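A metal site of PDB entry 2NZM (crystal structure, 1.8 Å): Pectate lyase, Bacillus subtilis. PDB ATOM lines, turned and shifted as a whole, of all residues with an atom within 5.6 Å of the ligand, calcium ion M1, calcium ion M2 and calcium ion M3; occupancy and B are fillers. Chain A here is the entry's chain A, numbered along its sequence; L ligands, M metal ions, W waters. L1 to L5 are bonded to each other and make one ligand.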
ATOM      1  N   LYS A 118      14.639  15.334  -2.260  1.00  0.00           N
ATOM      2  CA  LYS A 118      14.020  14.043  -2.603  1.00  0.00           C
ATOM      3  C   LYS A 118      15.044  12.916  -2.609  1.00  0.00           C
ATOM      4  O   LYS A 118      14.781  11.817  -2.120  1.00  0.00           O
ATOM      5  CB  LYS A 118      13.337  14.167  -3.965  1.00  0.00           C
ATOM      6  CG  LYS A 118      12.468  12.978  -4.376  1.00  0.00           C
ATOM      7  CD  LYS A 118      12.108  13.082  -5.838  1.00  0.00           C
ATOM      8  CE  LYS A 118      11.319  11.871  -6.310  1.00  0.00           C
ATOM      9  NZ  LYS A 118      11.053  11.971  -7.779  1.00  0.00           N
ATOM     10  N   GLN A 146       8.730   4.768   0.188  1.00  0.00           N
ATOM     11  CA  GLN A 146       7.843   4.471  -0.940  1.00  0.00           C
ATOM     12  C   GLN A 146       7.795   2.969  -1.207  1.00  0.00           C
ATOM     13  O   GLN A 146       8.839   2.310  -1.273  1.00  0.00           O
ATOM     14  CB  GLN A 146       8.271   5.229  -2.200  1.00  0.00           C
ATOM     15  CG  GLN A 146       7.415   4.878  -3.421  1.00  0.00           C
ATOM     16  CD  GLN A 146       7.682   5.747  -4.640  1.00  0.00           C
ATOM     17  OE1 GLN A 146       6.815   6.515  -5.058  1.00  0.00           O
ATOM     18  NE2 GLN A 146       8.881   5.621  -5.217  1.00  0.00           N
ATOM     19  N   ASP A 173      -5.387  25.931  -7.191  1.00  0.00           N
ATOM     20  CA  ASP A 173      -5.740  24.869  -6.268  1.00  0.00           C
ATOM     21  C   ASP A 173      -6.680  25.449  -5.210  1.00  0.00           C
ATOM     22  O   ASP A 173      -6.227  25.979  -4.183  1.00  0.00           O
ATOM     23  CB  ASP A 173      -4.487  24.240  -5.642  1.00  0.00           C
ATOM     24  CG  ASP A 173      -4.806  23.064  -4.736  1.00  0.00           C
ATOM     25  OD1 ASP A 173      -6.002  22.731  -4.573  1.00  0.00           O
ATOM     26  OD2 ASP A 173      -3.862  22.463  -4.179  1.00  0.00           O
ATOM     27  N   GLY A 174      -7.976  25.343  -5.460  1.00  0.00           N
ATOM     28  CA  GLY A 174      -8.976  26.000  -4.636  1.00  0.00           C
ATOM     29  C   GLY A 174      -9.203  27.424  -5.086  1.00  0.00           C
ATOM     30  O   GLY A 174      -8.436  27.962  -5.901  1.00  0.00           O
ATOM     31  N   ASN A 178      -3.360  27.338  -3.220  1.00  0.00           N
ATOM     32  CA  ASN A 178      -2.785  26.571  -2.109  1.00  0.00           C
ATOM     33  C   ASN A 178      -1.309  26.295  -2.357  1.00  0.00           C
ATOM     34  O   ASN A 178      -0.866  26.267  -3.503  1.00  0.00           O
ATOM     35  CB  ASN A 178      -3.518  25.237  -1.927  1.00  0.00           C
ATOM     36  CG  ASN A 178      -4.700  25.337  -0.984  1.00  0.00           C
ATOM     37  OD1 ASN A 178      -4.586  25.844   0.138  1.00  0.00           O
ATOM     38  ND2 ASN A 178      -5.849  24.841  -1.433  1.00  0.00           N
ATOM     39  N   ASN A 180       1.484  23.357  -2.012  1.00  0.00           N
ATOM     40  CA  ASN A 180       1.538  21.892  -1.976  1.00  0.00           C
ATOM     41  C   ASN A 180       2.968  21.376  -1.851  1.00  0.00           C
ATOM     42  O   ASN A 180       3.884  21.883  -2.511  1.00  0.00           O
ATOM     43  CB  ASN A 180       0.918  21.306  -3.253  1.00  0.00           C
ATOM     44  CG  ASN A 180      -0.577  21.548  -3.332  1.00  0.00           C
ATOM     45  OD1 ASN A 180      -1.361  20.884  -2.651  1.00  0.00           O
ATOM     46  ND2 ASN A 180      -0.985  22.470  -4.193  1.00  0.00           N
ATOM     47  N   SER A 181       3.149  20.371  -1.008  1.00  0.00           N
ATOM     48  CA  SER A 181       4.436  19.717  -0.820  1.00  0.00           C
ATOM     49  C   SER A 181       4.378  18.247  -1.236  1.00  0.00           C
ATOM     50  O   SER A 181       3.284  17.724  -1.524  1.00  0.00           O
ATOM     51  CB  SER A 181       4.895  19.862   0.636  1.00  0.00           C
ATOM     52  OG  SER A 181       5.418  21.164   0.862  1.00  0.00           O
ATOM     53  N   GLN A 182       5.528  17.593  -1.251  1.00  0.00           N
ATOM     54  CA  GLN A 182       5.671  16.290  -1.931  1.00  0.00           C
ATOM     55  C   GLN A 182       5.766  15.034  -1.052  1.00  0.00           C
ATOM     56  O   GLN A 182       5.466  13.933  -1.525  1.00  0.00           O
ATOM     57  CB  GLN A 182       6.885  16.338  -2.871  1.00  0.00           C
ATOM     58  CG  GLN A 182       6.682  17.212  -4.095  1.00  0.00           C
ATOM     59  CD  GLN A 182       5.552  16.721  -4.971  1.00  0.00           C
ATOM     60  OE1 GLN A 182       5.506  15.547  -5.358  1.00  0.00           O
ATOM     61  NE2 GLN A 182       4.626  17.618  -5.295  1.00  0.00           N
ATOM     62  N   TYR A 183       6.170  15.191   0.203  1.00  0.00           N
ATOM     63  CA  TYR A 183       6.564  14.011   0.990  1.00  0.00           C
ATOM     64  C   TYR A 183       5.506  13.526   1.954  1.00  0.00           C
ATOM     65  O   TYR A 183       4.986  14.304   2.742  1.00  0.00           O
ATOM     66  CB  TYR A 183       7.894  14.247   1.735  1.00  0.00           C
ATOM     67  CG  TYR A 183       8.952  14.815   0.815  1.00  0.00           C
ATOM     68  CD1 TYR A 183       9.320  14.140  -0.345  1.00  0.00           C
ATOM     69  CD2 TYR A 183       9.541  16.041   1.086  1.00  0.00           C
ATOM     70  CE1 TYR A 183      10.270  14.668  -1.210  1.00  0.00           C
ATOM     71  CE2 TYR A 183      10.494  16.584   0.230  1.00  0.00           C
ATOM     72  CZ  TYR A 183      10.850  15.894  -0.917  1.00  0.00           C
ATOM     73  OH  TYR A 183      11.785  16.422  -1.767  1.00  0.00           O
ATOM     74  N   ASP A 184       5.176  12.244   1.846  1.00  0.00           N
ATOM     75  CA  ASP A 184       4.367  11.543   2.838  1.00  0.00           C
ATOM     76  C   ASP A 184       5.315  10.783   3.753  1.00  0.00           C
ATOM     77  O   ASP A 184       6.489  10.635   3.443  1.00  0.00           O
ATOM     78  CB  ASP A 184       3.420  10.541   2.181  1.00  0.00           C
ATOM     79  CG  ASP A 184       2.731  11.080   0.947  1.00  0.00           C
ATOM     80  OD1 ASP A 184       2.283  12.254   0.960  1.00  0.00           O
ATOM     81  OD2 ASP A 184       2.624  10.313  -0.044  1.00  0.00           O
ATOM     82  N   THR A 187       4.370   6.300   1.145  1.00  0.00           N
ATOM     83  CA  THR A 187       3.633   6.378  -0.114  1.00  0.00           C
ATOM     84  C   THR A 187       3.573   4.994  -0.738  1.00  0.00           C
ATOM     85  O   THR A 187       4.602   4.411  -1.068  1.00  0.00           O
ATOM     86  CB  THR A 187       4.313   7.313  -1.127  1.00  0.00           C
ATOM     87  OG1 THR A 187       4.536   8.600  -0.536  1.00  0.00           O
ATOM     88  CG2 THR A 187       3.452   7.460  -2.374  1.00  0.00           C
ATOM     89  N   ASN A 189       2.885   3.390  -3.879  1.00  0.00           N
ATOM     90  CA  ASN A 189       2.807   3.737  -5.302  1.00  0.00           C
ATOM     91  C   ASN A 189       2.756   2.451  -6.146  1.00  0.00           C
ATOM     92  O   ASN A 189       3.772   1.981  -6.648  1.00  0.00           O
ATOM     93  CB  ASN A 189       4.014   4.616  -5.669  1.00  0.00           C
ATOM     94  CG  ASN A 189       3.972   5.123  -7.108  1.00  0.00           C
ATOM     95  OD1 ASN A 189       3.084   4.774  -7.890  1.00  0.00           O
ATOM     96  ND2 ASN A 189       4.939   5.969  -7.460  1.00  0.00           N
ATOM     97  N   ASP A 223       2.771  16.791   3.331  1.00  0.00           N
ATOM     98  CA  ASP A 223       1.772  16.233   2.450  1.00  0.00           C
ATOM     99  C   ASP A 223       0.964  15.193   3.224  1.00  0.00           C
ATOM    100  O   ASP A 223       0.328  15.523   4.232  1.00  0.00           O
ATOM    101  CB  ASP A 223       2.419  15.641   1.202  1.00  0.00           C
ATOM    102  CG  ASP A 223       1.431  15.452   0.086  1.00  0.00           C
ATOM    103  OD1 ASP A 223       0.673  16.405  -0.185  1.00  0.00           O
ATOM    104  OD2 ASP A 223       1.398  14.337  -0.506  1.00  0.00           O
ATOM    105  N   GLY A 224       1.029  13.946   2.781  1.00  0.00           N
ATOM    106  CA  GLY A 224       0.249  12.880   3.391  1.00  0.00           C
ATOM    107  C   GLY A 224       0.982  12.174   4.506  1.00  0.00           C
ATOM    108  O   GLY A 224       2.150  12.434   4.789  1.00  0.00           O
ATOM    109  N   ASP A 227      -0.366   7.505   2.096  1.00  0.00           N
ATOM    110  CA  ASP A 227      -1.097   7.647   0.834  1.00  0.00           C
ATOM    111  C   ASP A 227      -0.971   6.375  -0.002  1.00  0.00           C
ATOM    112  O   ASP A 227       0.011   5.633   0.132  1.00  0.00           O
ATOM    113  CB  ASP A 227      -0.559   8.827   0.023  1.00  0.00           C
ATOM    114  CG  ASP A 227      -0.937  10.187   0.615  1.00  0.00           C
ATOM    115  OD1 ASP A 227      -1.826  10.278   1.498  1.00  0.00           O
ATOM    116  OD2 ASP A 227      -0.341  11.197   0.165  1.00  0.00           O
ATOM    117  N   SER A 229      -1.680   5.037  -4.201  1.00  0.00           N
ATOM    118  CA  SER A 229      -1.880   5.550  -5.558  1.00  0.00           C
ATOM    119  C   SER A 229      -1.561   4.492  -6.600  1.00  0.00           C
ATOM    120  O   SER A 229      -0.977   3.455  -6.287  1.00  0.00           O
ATOM    121  CB  SER A 229      -0.958   6.765  -5.779  1.00  0.00           C
ATOM    122  OG  SER A 229      -1.230   7.383  -7.025  1.00  0.00           O
ATOM    123  N   ASN A 230      -1.984   4.752  -7.841  1.00  0.00           N
ATOM    124  CA  ASN A 230      -1.536   4.008  -9.013  1.00  0.00           C
ATOM    125  C   ASN A 230      -1.674   2.486  -8.908  1.00  0.00           C
ATOM    126  O   ASN A 230      -0.709   1.755  -9.097  1.00  0.00           O
ATOM    127  CB  ASN A 230      -0.096   4.394  -9.366  1.00  0.00           C
ATOM    128  CG  ASN A 230       0.030   5.872  -9.735  1.00  0.00           C
ATOM    129  OD1 ASN A 230      -0.894   6.456 -10.323  1.00  0.00           O
ATOM    130  ND2 ASN A 230       1.164   6.465  -9.383  1.00  0.00           N
ATOM    131  N   LYS A 247      -3.510  16.664   5.987  1.00  0.00           N
ATOM    132  CA  LYS A 247      -4.060  15.682   5.038  1.00  0.00           C
ATOM    133  C   LYS A 247      -3.467  14.301   5.294  1.00  0.00           C
ATOM    134  O   LYS A 247      -2.316  14.037   4.953  1.00  0.00           O
ATOM    135  CB  LYS A 247      -3.780  16.127   3.589  1.00  0.00           C
ATOM    136  CG  LYS A 247      -4.232  17.564   3.257  1.00  0.00           C
ATOM    137  CD  LYS A 247      -3.729  18.064   1.891  1.00  0.00           C
ATOM    138  CE  LYS A 247      -2.224  18.374   1.893  1.00  0.00           C
ATOM    139  NZ  LYS A 247      -1.789  19.195   0.715  1.00  0.00           N
ATOM    140  N   ILE A 250      -4.769   9.686   1.550  1.00  0.00           N
ATOM    141  CA  ILE A 250      -5.449   9.818   0.269  1.00  0.00           C
ATOM    142  C   ILE A 250      -5.219   8.537  -0.526  1.00  0.00           C
ATOM    143  O   ILE A 250      -4.077   8.179  -0.830  1.00  0.00           O
ATOM    144  CB  ILE A 250      -5.003  11.100  -0.481  1.00  0.00           C
ATOM    145  CG1 ILE A 250      -5.464  12.343   0.293  1.00  0.00           C
ATOM    146  CG2 ILE A 250      -5.565  11.116  -1.930  1.00  0.00           C
ATOM    147  CD1 ILE A 250      -5.076  13.665  -0.336  1.00  0.00           C
ATOM    148  N   GLY A 252      -6.059   6.770  -3.959  1.00  0.00           N
ATOM    149  CA  GLY A 252      -6.469   7.116  -5.310  1.00  0.00           C
ATOM    150  C   GLY A 252      -6.197   8.589  -5.511  1.00  0.00           C
ATOM    151  O   GLY A 252      -6.822   9.435  -4.870  1.00  0.00           O
ATOM    152  N   SER A 253      -5.251   8.891  -6.395  1.00  0.00           N
ATOM    153  CA  SER A 253      -4.695  10.237  -6.489  1.00  0.00           C
ATOM    154  C   SER A 253      -5.369  11.141  -7.538  1.00  0.00           C
ATOM    155  O   SER A 253      -5.102  12.346  -7.583  1.00  0.00           O
ATOM    156  CB  SER A 253      -3.188  10.166  -6.757  1.00  0.00           C
ATOM    157  OG  SER A 253      -2.935   9.742  -8.081  1.00  0.00           O
ATOM    158  N   SER A 254      -6.244  10.571  -8.371  1.00  0.00           N
ATOM    159  CA  SER A 254      -6.868  11.326  -9.461  1.00  0.00           C
ATOM    160  C   SER A 254      -8.164  10.726  -9.990  1.00  0.00           C
ATOM    161  O   SER A 254      -8.246   9.515 -10.210  1.00  0.00           O
ATOM    162  CB  SER A 254      -5.876  11.508 -10.625  1.00  0.00           C
ATOM    163  OG  SER A 254      -6.472  12.235 -11.682  1.00  0.00           O
ATOM    164  N   LYS A 257      -7.631   8.649 -13.172  1.00  0.00           N
ATOM    165  CA  LYS A 257      -6.987   7.333 -13.116  1.00  0.00           C
ATOM    166  C   LYS A 257      -8.010   6.214 -12.908  1.00  0.00           C
ATOM    167  O   LYS A 257      -8.064   5.572 -11.847  1.00  0.00           O
ATOM    168  CB  LYS A 257      -5.899   7.311 -12.025  1.00  0.00           C
ATOM    169  CG  LYS A 257      -4.616   8.035 -12.402  1.00  0.00           C
ATOM    170  CD  LYS A 257      -3.828   8.412 -11.159  1.00  0.00           C
ATOM    171  CE  LYS A 257      -2.715   9.409 -11.480  1.00  0.00           C
ATOM    172  NZ  LYS A 257      -1.407   8.733 -11.731  1.00  0.00           N
ATOM    173  N   GLN A 278      -8.191  16.402   7.733  1.00  0.00           N
ATOM    174  CA  GLN A 278      -8.979  15.818   6.662  1.00  0.00           C
ATOM    175  C   GLN A 278      -8.351  14.569   6.063  1.00  0.00           C
ATOM    176  O   GLN A 278      -7.196  14.217   6.378  1.00  0.00           O
ATOM    177  CB  GLN A 278      -9.190  16.857   5.549  1.00  0.00           C
ATOM    178  CG  GLN A 278      -7.903  17.340   4.895  1.00  0.00           C
ATOM    179  CD  GLN A 278      -8.137  18.555   4.017  1.00  0.00           C
ATOM    180  OE1 GLN A 278      -9.033  18.550   3.178  1.00  0.00           O
ATOM    181  NE2 GLN A 278      -7.351  19.596   4.221  1.00  0.00           N
ATOM    182  N   ARG A 282      -9.464   9.824   2.420  1.00  0.00           N
ATOM    183  CA  ARG A 282     -10.150  10.320   1.219  1.00  0.00           C
ATOM    184  C   ARG A 282      -9.976   9.255   0.151  1.00  0.00           C
ATOM    185  O   ARG A 282      -8.848   8.890  -0.181  1.00  0.00           O
ATOM    186  CB  ARG A 282      -9.550  11.640   0.748  1.00  0.00           C
ATOM    187  CG  ARG A 282     -10.334  12.303  -0.396  1.00  0.00           C
ATOM    188  CD  ARG A 282      -9.408  13.106  -1.307  1.00  0.00           C
ATOM    189  NE  ARG A 282     -10.144  14.006  -2.210  1.00  0.00           N
ATOM    190  CZ  ARG A 282     -10.792  13.619  -3.305  1.00  0.00           C
ATOM    191  NH1 ARG A 282     -10.827  12.344  -3.661  1.00  0.00           N
ATOM    192  NH2 ARG A 282     -11.413  14.538  -4.057  1.00  0.00           N
ATOM    193  N   ARG A 284     -10.880   7.511  -3.715  1.00  0.00           N
ATOM    194  CA  ARG A 284     -11.416   7.381  -5.070  1.00  0.00           C
ATOM    195  C   ARG A 284     -11.416   5.897  -5.428  1.00  0.00           C
ATOM    196  O   ARG A 284     -10.456   5.193  -5.096  1.00  0.00           O
ATOM    197  CB  ARG A 284     -10.540   8.152  -6.067  1.00  0.00           C
ATOM    198  CG  ARG A 284     -10.517   9.679  -5.892  1.00  0.00           C
ATOM    199  CD  ARG A 284      -9.454  10.307  -6.798  1.00  0.00           C
ATOM    200  NE  ARG A 284      -9.517  11.767  -6.824  1.00  0.00           N
ATOM    201  CZ  ARG A 284      -8.731  12.587  -6.110  1.00  0.00           C
ATOM    202  NH1 ARG A 284      -7.801  12.114  -5.291  1.00  0.00           N
ATOM    203  NH2 ARG A 284      -8.910  13.892  -6.212  1.00  0.00           N
ATOM    204  N   TYR A 308     -13.202  17.070   7.976  1.00  0.00           N
ATOM    205  CA  TYR A 308     -13.995  15.856   7.749  1.00  0.00           C
ATOM    206  C   TYR A 308     -13.184  14.600   8.068  1.00  0.00           C
ATOM    207  O   TYR A 308     -11.954  14.668   8.121  1.00  0.00           O
ATOM    208  CB  TYR A 308     -14.553  15.801   6.319  1.00  0.00           C
ATOM    209  CG  TYR A 308     -13.545  15.488   5.225  1.00  0.00           C
ATOM    210  CD1 TYR A 308     -13.242  14.168   4.884  1.00  0.00           C
ATOM    211  CD2 TYR A 308     -12.905  16.509   4.521  1.00  0.00           C
ATOM    212  CE1 TYR A 308     -12.324  13.872   3.891  1.00  0.00           C
ATOM    213  CE2 TYR A 308     -11.985  16.217   3.510  1.00  0.00           C
ATOM    214  CZ  TYR A 308     -11.701  14.892   3.202  1.00  0.00           C
ATOM    215  OH  TYR A 308     -10.806  14.590   2.203  1.00  0.00           O
ATOM    216  N   PHE A 339     -17.390  14.357  -2.703  1.00  0.00           N
ATOM    217  CA  PHE A 339     -16.808  14.986  -3.884  1.00  0.00           C
ATOM    218  C   PHE A 339     -17.524  14.500  -5.137  1.00  0.00           C
ATOM    219  O   PHE A 339     -18.193  13.472  -5.120  1.00  0.00           O
ATOM    220  CB  PHE A 339     -15.315  14.684  -3.963  1.00  0.00           C
ATOM    221  CG  PHE A 339     -14.530  15.161  -2.775  1.00  0.00           C
ATOM    222  CD1 PHE A 339     -14.037  16.471  -2.718  1.00  0.00           C
ATOM    223  CD2 PHE A 339     -14.297  14.316  -1.685  1.00  0.00           C
ATOM    224  CE1 PHE A 339     -13.318  16.925  -1.604  1.00  0.00           C
ATOM    225  CE2 PHE A 339     -13.586  14.760  -0.574  1.00  0.00           C
ATOM    226  CZ  PHE A 339     -13.094  16.064  -0.530  1.00  0.00           C
HETATM  227  C1  LIG L   1      -8.323  20.102   0.008  1.00  0.00           C
HETATM  228  C2  LIG L   1      -7.072  20.466  -0.805  1.00  0.00           C
HETATM  229  C3  LIG L   1      -7.403  20.500  -2.286  1.00  0.00           C
HETATM  230  C4  LIG L   1      -8.060  19.195  -2.745  1.00  0.00           C
HETATM  231  C5  LIG L   1      -9.244  18.806  -1.840  1.00  0.00           C
HETATM  232  C6  LIG L   1      -9.703  17.420  -2.186  1.00  0.00           C
HETATM  233  O1  LIG L   1      -9.289  21.157  -0.104  1.00  0.00           O
HETATM  234  O2  LIG L   1      -6.585  21.747  -0.372  1.00  0.00           O
HETATM  235  O3  LIG L   1      -6.194  20.764  -3.014  1.00  0.00           O
HETATM  236  O4  LIG L   1      -7.117  18.101  -2.747  1.00  0.00           O
HETATM  237  O5  LIG L   1      -8.866  18.854  -0.459  1.00  0.00           O
HETATM  238  O6  LIG L   1     -10.047  17.200  -3.364  1.00  0.00           O
HETATM  239  O7  LIG L   1      -9.717  16.535  -1.298  1.00  0.00           O
HETATM  240  C1  LG2 L   2      -6.311  17.867  -3.908  1.00  0.00           C
HETATM  241  C2  LG2 L   2      -6.496  16.521  -4.598  1.00  0.00           C
HETATM  242  C3  LG2 L   2      -6.032  15.372  -3.688  1.00  0.00           C
HETATM  243  C4  LG2 L   2      -4.643  15.673  -3.135  1.00  0.00           C
HETATM  244  C5  LG2 L   2      -4.651  17.019  -2.397  1.00  0.00           C
HETATM  245  C6  LG2 L   2      -3.360  17.388  -1.703  1.00  0.00           C
HETATM  246  O1  LG2 L   2      -7.880  16.379  -4.940  1.00  0.00           O
HETATM  247  O2  LG2 L   2      -6.043  14.141  -4.424  1.00  0.00           O
HETATM  248  O3  LG2 L   2      -3.730  15.687  -4.241  1.00  0.00           O
HETATM  249  O4  LG2 L   2      -4.982  18.026  -3.360  1.00  0.00           O
HETATM  250  O5  LG2 L   2      -2.684  16.488  -1.149  1.00  0.00           O
HETATM  251  O6  LG2 L   2      -3.011  18.591  -1.671  1.00  0.00           O
HETATM  252  C1  LG3 L   3      -2.372  16.080  -4.542  1.00  0.00           C
HETATM  253  C2  LG3 L   3      -2.001  16.174  -6.015  1.00  0.00           C
HETATM  254  C3  LG3 L   3      -2.165  14.805  -6.667  1.00  0.00           C
HETATM  255  C4  LG3 L   3      -1.397  13.736  -5.896  1.00  0.00           C
HETATM  256  C5  LG3 L   3      -1.828  13.735  -4.420  1.00  0.00           C
HETATM  257  C6  LG3 L   3      -1.028  12.766  -3.598  1.00  0.00           C
HETATM  258  O1  LG3 L   3      -2.845  17.138  -6.653  1.00  0.00           O
HETATM  259  O2  LG3 L   3      -1.724  14.857  -8.033  1.00  0.00           O
HETATM  260  O3  LG3 L   3       0.020  13.979  -5.981  1.00  0.00           O
HETATM  261  O4  LG3 L   3      -1.640  15.043  -3.882  1.00  0.00           O
HETATM  262  O5  LG3 L   3      -1.133  11.542  -3.836  1.00  0.00           O
HETATM  263  O6  LG3 L   3      -0.299  13.225  -2.690  1.00  0.00           O
HETATM  264  C1  LG4 L   4       1.047  13.028  -6.297  1.00  0.00           C
HETATM  265  C2  LG4 L   4       2.452  13.528  -6.633  1.00  0.00           C
HETATM  266  C3  LG4 L   4       2.475  14.065  -8.069  1.00  0.00           C
HETATM  267  C4  LG4 L   4       1.895  13.059  -9.070  1.00  0.00           C
HETATM  268  C5  LG4 L   4       0.564  12.487  -8.585  1.00  0.00           C
HETATM  269  C6  LG4 L   4       0.089  11.367  -9.474  1.00  0.00           C
HETATM  270  O1  LG4 L   4       2.835  14.564  -5.710  1.00  0.00           O
HETATM  271  O2  LG4 L   4       3.829  14.393  -8.429  1.00  0.00           O
HETATM  272  O3  LG4 L   4       2.827  11.998  -9.304  1.00  0.00           O
HETATM  273  O4  LG4 L   4       0.676  12.006  -7.232  1.00  0.00           O
HETATM  274  O5  LG4 L   4      -0.233  11.650 -10.650  1.00  0.00           O
HETATM  275  O6  LG4 L   4       0.025  10.206  -9.017  1.00  0.00           O
HETATM  276  C1  LG5 L   5       3.852  11.393 -10.119  1.00  0.00           C
HETATM  277  C2  LG5 L   5       3.875   9.864 -10.156  1.00  0.00           C
HETATM  278  C3  LG5 L   5       4.738   9.284  -9.030  1.00  0.00           C
HETATM  279  C4  LG5 L   5       6.081  10.013  -8.847  1.00  0.00           C
HETATM  280  C5  LG5 L   5       5.944  11.533  -8.964  1.00  0.00           C
HETATM  281  C6  LG5 L   5       7.303  12.185  -9.025  1.00  0.00           C
HETATM  282  O1  LG5 L   5       2.544   9.361 -10.033  1.00  0.00           O
HETATM  283  O2  LG5 L   5       4.972   7.900  -9.323  1.00  0.00           O
HETATM  284  O3  LG5 L   5       7.040   9.526  -9.797  1.00  0.00           O
HETATM  285  O4  LG5 L   5       5.191  11.906 -10.125  1.00  0.00           O
HETATM  286  O5  LG5 L   5       7.864  12.499  -7.946  1.00  0.00           O
HETATM  287  O6  LG5 L   5       7.822  12.383 -10.137  1.00  0.00           O
HETATM  288 CA    CA M   1       1.336  12.105  -1.157  1.00  0.00          CA
HETATM  289 CA    CA M   2      -3.698  20.306  -3.080  1.00  0.00          CA
HETATM  290 CA    CA M   3      -0.529  15.402  -1.886  1.00  0.00          CA
HETATM  291  O   HOH W   1      -0.308  17.886  -2.804  1.00  0.00           O
HETATM  292  O   HOH W   2       6.011  10.762 -12.768  1.00  0.00           O
HETATM  293  O   HOH W   3      -2.657  13.027  -9.735  1.00  0.00           O
HETATM  294  O   HOH W   4     -10.422  23.477   0.776  1.00  0.00           O
HETATM  295  O   HOH W   5       0.982  10.294  -2.978  1.00  0.00           O
HETATM  296  O   HOH W   6      -7.836  16.640  -7.748  1.00  0.00           O
HETATM  297  O   HOH W   7     -11.663  19.891   0.083  1.00  0.00           O
HETATM  298  O   HOH W   8      -8.060  22.340   2.528  1.00  0.00           O
HETATM  299  O   HOH W   9      -9.274  16.505   1.311  1.00  0.00           O
HETATM  300  O   HOH W  10     -11.353  18.884  -4.937  1.00  0.00           O
HETATM  301  O   HOH W  11       9.753   9.152  -9.792  1.00  0.00           O
HETATM  302  O   HOH W  12      -8.350  23.709  -1.775  1.00  0.00           O
HETATM  303  O   HOH W  13       1.670  16.014  -3.182  1.00  0.00           O
HETATM  304  O   HOH W  14       9.181  13.494 -12.613  1.00  0.00           O
HETATM  305  O   HOH W  15      -3.146  19.726  -5.264  1.00  0.00           O
HETATM  306  O   HOH W  16      -5.393  22.525   2.356  1.00  0.00           O
HETATM  307  O   HOH W  17       1.763   8.779  -6.850  1.00  0.00           O
HETATM  308  O   HOH W  18       6.495  13.103  -5.657  1.00  0.00           O
HETATM  309  O   HOH W  19      -5.175  16.328  -8.039  1.00  0.00           O
HETATM  310  O   HOH W  20      -1.597  13.947  -0.220  1.00  0.00           O
HETATM  311  O   HOH W  21       3.349  12.651  -2.487  1.00  0.00           O
HETATM  312  O   HOH W  22      -2.486   9.167  -3.275  1.00  0.00           O
HETATM  313  O   HOH W  23      -3.935  21.630  -1.103  1.00  0.00           O
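Two residues have an atom within 4 Å of calcium ion M2: Asp 173 and Asn 180.
The nearest printed residue that does not touch calcium ion M2 is Lys 247 (4.4 Å).
OG of Ser 229 touches O6 of LG4 L4, 3.7 Å away.
CD1 of Ile 250 touches C4 of LG2 L2, at 3.5 Å.
Gln 278 touches the ligand.
CZ of Phe 339 touches O7 of LIG L1, 3.5 Å away.
Of the 28 residues printed, 18 come within 4 Å of the ligand.
Along chain A the residues within 4 Å of the ligand span positions 118 to 339.
Calcium ion M1 is bound by the side-chain carboxylate (OD2) of Asp 227 (2.3 Å), the side-chain carboxylate (OD1) of Asp 184 (2.3 Å), the side-chain carboxylate (OD2) of Asp 223 (2.3 Å), the side-chain carboxylate (OD2) of Asp 184 (2.5 Å), water W21 (2.5 Å), an oxygen (O6) of LG3 L3 (2.5 Å) and water W5 (2.6 Å).
Calcium ion M1 has seven donor atoms within binding distance.
The side-chain amide nitrogen (ND2) of Asn 189 sits at hydrogen-bond distance from an oxygen (O2) of LG5 L5 (2.7 Å).
The guanidinium group (NE) of Arg 282 is in salt-bridge range of an oxygen (O7) of LIG L1, 2.7 Å away.
An oxygen (O6) of LG2 L2 lies close to the side-chain amino group (NZ) of Lys 247, at 2.7 Å.
An oxygen (O2) of LG2 L2 lies within hydrogen-bond range of the guanidinium group (NH1) of Arg 284 (2.8 Å).
O1 of LG4 L4 is in hydrogen-bond range of OE1 of Gln 182, 2.9 Å away.
An oxygen (O6) of LG4 L4 is in hydrogen-bond range of the side-chain hydroxyl (OG) of Ser 253 (3.1 Å).
An oxygen (O5) of LG5 L5 is in salt-bridge range of the side-chain amino group (NZ) of Lys 118 (3.2 Å).
An oxygen (O1) of LG5 L5 sits at hydrogen-bond distance from the side-chain amide nitrogen (ND2) of Asn 230 (3.3 Å).
The side-chain amino group (NZ) of Lys 257 is in salt-bridge range of an oxygen (O5) of LG4 L4 (3.3 Å).
O2 of LIG L1 sits at hydrogen-bond distance from ND2 of Asn 178.
Calcium ion M2 is bound by an oxygen (O6) of LG2 L2, water W15, water W23, the side-chain carboxylate (OD2) of Asp 173, the side-chain amide oxygen (OD1) of Asn 180, an oxygen (O3) of LIG L1 and an oxygen (O4) of LG2 L2.
Calcium ion M3 is bound by OD1 of Asp 223 (2.3 Å), O4 of LG3 L3 (2.3 Å), O6 of LG3 L3 (2.3 Å), water W20 (2.5 Å), O5 of LG2 L2 (2.5 Å), OD2 of Asp 223 (2.6 Å), water W13 (2.6 Å) and water W1 (2.7 Å).
Of the 28 residues printed, 3 come within 4 Å of calcium ion M1.
Water W13 lies within hydrogen-bond range of O of Ser 181 (2.9 Å) and O1 of LG4 L4 (3.1 Å).
Water W9 lies within hydrogen-bond range of the side-chain hydroxyl (OH) of Tyr 308 (2.6 Å), an oxygen (O7) of LIG L1 (2.6 Å) and the side-chain amide oxygen (OE1) of Gln 278 (2.8 Å).
Water W3 lies within hydrogen-bond range of O2 of LG3 L3 (2.7 Å) and O of Ser 253 (3.3 Å).
Water W18 lies within hydrogen-bond range of OE1 of Gln 182 and O5 of LG5 L5.
Water W22 lies within hydrogen-bond range of an oxygen (O5) of LG3 L3 (2.8 Å) and the backbone carbonyl oxygen (O) of Ile 250 (3.1 Å).
Water W8 lies within hydrogen-bond range of O1 of LIG L1 (3.1 Å) and NE2 of Gln 278 (3.3 Å).
OD1 of Asp 223 sits close to NZ of Lys 247 (3.8 Å).
OD1 of Asp 227 lies within hydrogen-bond range of N of Ile 250.
The side-chain carboxylate of Asp 184 sits close to the backbone NH of Gly 224, 2.8 Å away.
The side-chain carboxylate (OD2) of Asp 184 lies close to the side-chain hydroxyl (OG1) of Thr 187 (2.6 Å).
O of Asp 173 lies within hydrogen-bond range of ND2 of Asn 178.
OD1 of Asn 189 lies within hydrogen-bond range of ND2 of Asn 230 (3.0 Å).
The backbone NH (N) of Lys 118 is in hydrogen-bond range of the side-chain hydroxyl (OH) of Tyr 183, 3.1 Å away.
The side-chain amide oxygen of Asn 230 sits close to the side-chain hydroxyl of Ser 229 (3.4 Å).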
